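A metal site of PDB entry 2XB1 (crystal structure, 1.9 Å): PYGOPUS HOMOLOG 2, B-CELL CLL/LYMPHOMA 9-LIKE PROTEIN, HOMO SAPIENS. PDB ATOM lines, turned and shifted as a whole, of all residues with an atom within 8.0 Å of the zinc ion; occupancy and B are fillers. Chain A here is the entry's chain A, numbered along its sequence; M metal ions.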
ATOM      1  N   PRO A   5      13.173 -20.793  22.880  1.00  0.00           N
ATOM      2  CA  PRO A   5      12.775 -20.415  21.508  1.00  0.00           C
ATOM      3  C   PRO A   5      11.580 -19.447  21.503  1.00  0.00           C
ATOM      4  O   PRO A   5      10.633 -19.653  22.276  1.00  0.00           O
ATOM      5  CB  PRO A   5      12.389 -21.746  20.847  1.00  0.00           C
ATOM      6  CG  PRO A   5      13.017 -22.838  21.735  1.00  0.00           C
ATOM      7  CD  PRO A   5      12.971 -22.242  23.133  1.00  0.00           C
ATOM      8  N   CYS A   6      11.656 -18.388  20.695  1.00  0.00           N
ATOM      9  CA  CYS A   6      10.538 -17.468  20.512  1.00  0.00           C
ATOM     10  C   CYS A   6       9.304 -18.220  20.064  1.00  0.00           C
ATOM     11  O   CYS A   6       9.344 -19.039  19.103  1.00  0.00           O
ATOM     12  CB  CYS A   6      10.883 -16.363  19.476  1.00  0.00           C
ATOM     13  SG  CYS A   6       9.505 -15.179  19.205  1.00  0.00           S
ATOM     14  N   GLY A   7       8.182 -17.914  20.700  1.00  0.00           N
ATOM     15  CA  GLY A   7       6.934 -18.567  20.349  1.00  0.00           C
ATOM     16  C   GLY A   7       6.414 -18.236  18.961  1.00  0.00           C
ATOM     17  O   GLY A   7       5.521 -18.929  18.453  1.00  0.00           O
ATOM     18  N   ALA A   8       6.934 -17.165  18.342  1.00  0.00           N
ATOM     19  CA  ALA A   8       6.468 -16.761  17.011  1.00  0.00           C
ATOM     20  C   ALA A   8       7.530 -17.069  15.920  1.00  0.00           C
ATOM     21  O   ALA A   8       7.235 -17.765  14.934  1.00  0.00           O
ATOM     22  CB  ALA A   8       6.092 -15.242  16.977  1.00  0.00           C
ATOM     23  N   CYS A   9       8.777 -16.617  16.110  1.00  0.00           N
ATOM     24  CA  CYS A   9       9.797 -16.770  15.014  1.00  0.00           C
ATOM     25  C   CYS A   9      10.701 -17.979  15.202  1.00  0.00           C
ATOM     26  O   CYS A   9      11.448 -18.361  14.294  1.00  0.00           O
ATOM     27  CB  CYS A   9      10.647 -15.510  14.860  1.00  0.00           C
ATOM     28  SG  CYS A   9      11.929 -15.337  16.151  1.00  0.00           S
ATOM     29  N   ARG A  10      10.618 -18.590  16.391  1.00  0.00           N
ATOM     30  CA  ARG A  10      11.356 -19.785  16.765  1.00  0.00           C
ATOM     31  C   ARG A  10      12.861 -19.647  17.036  1.00  0.00           C
ATOM     32  O   ARG A  10      13.485 -20.660  17.374  1.00  0.00           O
ATOM     33  CB  ARG A  10      11.120 -20.948  15.765  1.00  0.00           C
ATOM     34  CG  ARG A  10       9.652 -21.276  15.451  1.00  0.00           C
ATOM     35  CD  ARG A  10       9.617 -22.536  14.510  1.00  0.00           C
ATOM     36  NE  ARG A  10       9.653 -22.219  13.070  1.00  0.00           N
ATOM     37  CZ  ARG A  10      10.560 -22.669  12.189  1.00  0.00           C
ATOM     38  NH1 ARG A  10      11.557 -23.458  12.572  1.00  0.00           N
ATOM     39  NH2 ARG A  10      10.484 -22.327  10.910  1.00  0.00           N
ATOM     40  N   SER A  11      13.469 -18.458  16.889  1.00  0.00           N
ATOM     41  CA  SER A  11      14.873 -18.355  17.266  1.00  0.00           C
ATOM     42  C   SER A  11      14.990 -18.026  18.764  1.00  0.00           C
ATOM     43  O   SER A  11      13.999 -17.619  19.401  1.00  0.00           O
ATOM     44  CB  SER A  11      15.681 -17.365  16.402  1.00  0.00           C
ATOM     45  OG  SER A  11      15.143 -16.059  16.497  1.00  0.00           O
ATOM     46  N   GLU A  12      16.191 -18.255  19.306  1.00  0.00           N
ATOM     47  CA  GLU A  12      16.457 -18.088  20.734  1.00  0.00           C
ATOM     48  C   GLU A  12      16.099 -16.683  21.235  1.00  0.00           C
ATOM     49  O   GLU A  12      16.391 -15.669  20.577  1.00  0.00           O
ATOM     50  CB  GLU A  12      17.928 -18.421  21.054  1.00  0.00           C
ATOM     51  CG  GLU A  12      18.412 -18.029  22.444  1.00  0.00           C
ATOM     52  CD  GLU A  12      19.700 -18.734  22.884  1.00  0.00           C
ATOM     53  OE1 GLU A  12      20.279 -19.487  22.077  1.00  0.00           O
ATOM     54  OE2 GLU A  12      20.099 -18.557  24.057  1.00  0.00           O
ATOM     55  N   VAL A  13      15.433 -16.641  22.383  1.00  0.00           N
ATOM     56  CA  VAL A  13      15.193 -15.395  23.076  1.00  0.00           C
ATOM     57  C   VAL A  13      16.302 -15.209  24.144  1.00  0.00           C
ATOM     58  O   VAL A  13      16.425 -16.015  25.069  1.00  0.00           O
ATOM     59  CB  VAL A  13      13.800 -15.374  23.725  1.00  0.00           C
ATOM     60  CG1 VAL A  13      13.593 -14.038  24.482  1.00  0.00           C
ATOM     61  CG2 VAL A  13      12.732 -15.515  22.625  1.00  0.00           C
ATOM     62  N   GLN A  17      17.527  -9.115  24.895  1.00  0.00           N
ATOM     63  CA  GLN A  17      16.412  -8.771  23.970  1.00  0.00           C
ATOM     64  C   GLN A  17      15.136  -8.485  24.763  1.00  0.00           C
ATOM     65  O   GLN A  17      14.834  -9.264  25.691  1.00  0.00           O
ATOM     66  CB  GLN A  17      16.167  -9.976  23.040  1.00  0.00           C
ATOM     67  CG  GLN A  17      17.378 -10.302  22.139  1.00  0.00           C
ATOM     68  CD  GLN A  17      17.116 -11.505  21.234  1.00  0.00           C
ATOM     69  OE1 GLN A  17      16.703 -12.584  21.698  1.00  0.00           O
ATOM     70  NE2 GLN A  17      17.353 -11.320  19.958  1.00  0.00           N
ATOM     71  N   ASP A  18      14.387  -7.430  24.422  1.00  0.00           N
ATOM     72  CA  ASP A  18      13.005  -7.183  24.984  1.00  0.00           C
ATOM     73  C   ASP A  18      12.188  -8.426  24.672  1.00  0.00           C
ATOM     74  O   ASP A  18      12.107  -8.837  23.497  1.00  0.00           O
ATOM     75  CB  ASP A  18      12.252  -6.071  24.250  1.00  0.00           C
ATOM     76  CG  ASP A  18      12.834  -4.644  24.458  1.00  0.00           C
ATOM     77  OD1 ASP A  18      13.708  -4.452  25.323  1.00  0.00           O
ATOM     78  OD2 ASP A  18      12.347  -3.703  23.758  1.00  0.00           O
ATOM     79  N   TRP A  29       8.419 -17.766  25.745  1.00  0.00           N
ATOM     80  CA  TRP A  29       8.904 -16.400  25.570  1.00  0.00           C
ATOM     81  C   TRP A  29       8.699 -15.904  24.129  1.00  0.00           C
ATOM     82  O   TRP A  29       8.708 -16.724  23.212  1.00  0.00           O
ATOM     83  CB  TRP A  29      10.405 -16.331  25.935  1.00  0.00           C
ATOM     84  CG  TRP A  29      10.602 -16.360  27.401  1.00  0.00           C
ATOM     85  CD1 TRP A  29      10.855 -17.488  28.199  1.00  0.00           C
ATOM     86  CD2 TRP A  29      10.582 -15.247  28.289  1.00  0.00           C
ATOM     87  NE1 TRP A  29      10.970 -17.112  29.530  1.00  0.00           N
ATOM     88  CE2 TRP A  29      10.826 -15.749  29.611  1.00  0.00           C
ATOM     89  CE3 TRP A  29      10.364 -13.860  28.120  1.00  0.00           C
ATOM     90  CZ2 TRP A  29      10.868 -14.913  30.731  1.00  0.00           C
ATOM     91  CZ3 TRP A  29      10.411 -13.027  29.232  1.00  0.00           C
ATOM     92  CH2 TRP A  29      10.654 -13.554  30.528  1.00  0.00           C
ATOM     93  N   PHE A  30       8.497 -14.604  23.929  1.00  0.00           N
ATOM     94  CA  PHE A  30       8.307 -14.018  22.578  1.00  0.00           C
ATOM     95  C   PHE A  30       9.166 -12.763  22.546  1.00  0.00           C
ATOM     96  O   PHE A  30       9.085 -11.927  23.460  1.00  0.00           O
ATOM     97  CB  PHE A  30       6.833 -13.583  22.324  1.00  0.00           C
ATOM     98  CG  PHE A  30       5.856 -14.730  22.113  1.00  0.00           C
ATOM     99  CD1 PHE A  30       5.362 -15.025  20.834  1.00  0.00           C
ATOM    100  CD2 PHE A  30       5.454 -15.531  23.176  1.00  0.00           C
ATOM    101  CE1 PHE A  30       4.431 -16.069  20.642  1.00  0.00           C
ATOM    102  CE2 PHE A  30       4.549 -16.607  22.996  1.00  0.00           C
ATOM    103  CZ  PHE A  30       4.024 -16.865  21.759  1.00  0.00           C
ATOM    104  N   HIS A  31       9.977 -12.599  21.483  1.00  0.00           N
ATOM    105  CA  HIS A  31      10.602 -11.276  21.250  1.00  0.00           C
ATOM    106  C   HIS A  31       9.500 -10.242  21.160  1.00  0.00           C
ATOM    107  O   HIS A  31       8.485 -10.500  20.485  1.00  0.00           O
ATOM    108  CB  HIS A  31      11.428 -11.214  19.963  1.00  0.00           C
ATOM    109  CG  HIS A  31      12.479 -12.265  19.828  1.00  0.00           C
ATOM    110  ND1 HIS A  31      12.350 -13.343  18.963  1.00  0.00           N
ATOM    111  CD2 HIS A  31      13.698 -12.382  20.418  1.00  0.00           C
ATOM    112  CE1 HIS A  31      13.466 -14.065  19.028  1.00  0.00           C
ATOM    113  NE2 HIS A  31      14.269 -13.533  19.936  1.00  0.00           N
ATOM    114  N   ARG A  32       9.676  -9.067  21.780  1.00  0.00           N
ATOM    115  CA  ARG A  32       8.669  -8.015  21.716  1.00  0.00           C
ATOM    116  C   ARG A  32       8.259  -7.716  20.262  1.00  0.00           C
ATOM    117  O   ARG A  32       7.076  -7.608  19.970  1.00  0.00           O
ATOM    118  CB  ARG A  32       9.142  -6.747  22.393  1.00  0.00           C
ATOM    119  CG  ARG A  32       8.142  -5.577  22.278  1.00  0.00           C
ATOM    120  CD  ARG A  32       8.737  -4.252  22.863  1.00  0.00           C
ATOM    121  NE  ARG A  32       9.785  -3.725  21.975  1.00  0.00           N
ATOM    122  CZ  ARG A  32       9.537  -2.992  20.892  1.00  0.00           C
ATOM    123  NH1 ARG A  32       8.275  -2.702  20.556  1.00  0.00           N
ATOM    124  NH2 ARG A  32      10.524  -2.518  20.134  1.00  0.00           N
ATOM    125  N   GLU A  33       9.235  -7.497  19.383  1.00  0.00           N
ATOM    126  CA  GLU A  33       8.919  -7.129  18.006  1.00  0.00           C
ATOM    127  C   GLU A  33       8.257  -8.260  17.193  1.00  0.00           C
ATOM    128  O   GLU A  33       7.723  -8.025  16.088  1.00  0.00           O
ATOM    129  CB  GLU A  33      10.191  -6.577  17.328  1.00  0.00           C
ATOM    130  CG  GLU A  33      10.587  -5.251  18.053  1.00  0.00           C
ATOM    131  CD  GLU A  33      11.571  -4.365  17.296  1.00  0.00           C
ATOM    132  OE1 GLU A  33      11.139  -3.642  16.340  1.00  0.00           O
ATOM    133  OE2 GLU A  33      12.770  -4.334  17.686  1.00  0.00           O
ATOM    134  N   CYS A  34       8.269  -9.489  17.709  1.00  0.00           N
ATOM    135  CA  CYS A  34       7.499 -10.586  17.100  1.00  0.00           C
ATOM    136  C   CYS A  34       6.011 -10.587  17.481  1.00  0.00           C
ATOM    137  O   CYS A  34       5.268 -11.453  16.987  1.00  0.00           O
ATOM    138  CB  CYS A  34       8.144 -11.950  17.434  1.00  0.00           C
ATOM    139  SG  CYS A  34       9.805 -12.158  16.662  1.00  0.00           S
ATOM    140  N   THR A  35       5.597  -9.704  18.409  1.00  0.00           N
ATOM    141  CA  THR A  35       4.196  -9.705  18.947  1.00  0.00           C
ATOM    142  C   THR A  35       3.373  -8.524  18.458  1.00  0.00           C
ATOM    143  O   THR A  35       2.148  -8.588  18.508  1.00  0.00           O
ATOM    144  CB  THR A  35       4.137  -9.718  20.487  1.00  0.00           C
ATOM    145  OG1 THR A  35       4.646  -8.480  20.983  1.00  0.00           O
ATOM    146  CG2 THR A  35       4.969 -10.928  21.072  1.00  0.00           C
HETATM  147 ZN    ZN M   1      10.847 -13.924  17.728  1.00  0.00          ZN
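The zinc ion is bound by ND1 of His 31, SG of Cys 34, SG of Cys 6 and SG of Cys 9.
Four residues have an atom within 4 Å of the zinc ion: Cys 6, Cys 9, His 31 and Cys 34.
A ring nitrogen (NE2) of His 31 sits at hydrogen-bond distance from the backbone carbonyl oxygen (O) of Glu 12 (3.1 Å).
A ring nitrogen (NE2) of His 31 is in hydrogen-bond range of the side-chain amide oxygen (OE1) of Gln 17, 3.2 Å away.
SG of Cys 6 sits close to N of Ala 8.
The backbone NH (N) of Cys 6 sits at hydrogen-bond distance from the backbone carbonyl oxygen (O) of Ser 11 (2.8 Å).
OG of Ser 11 lies close to SG of Cys 9, 3.3 Å away.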
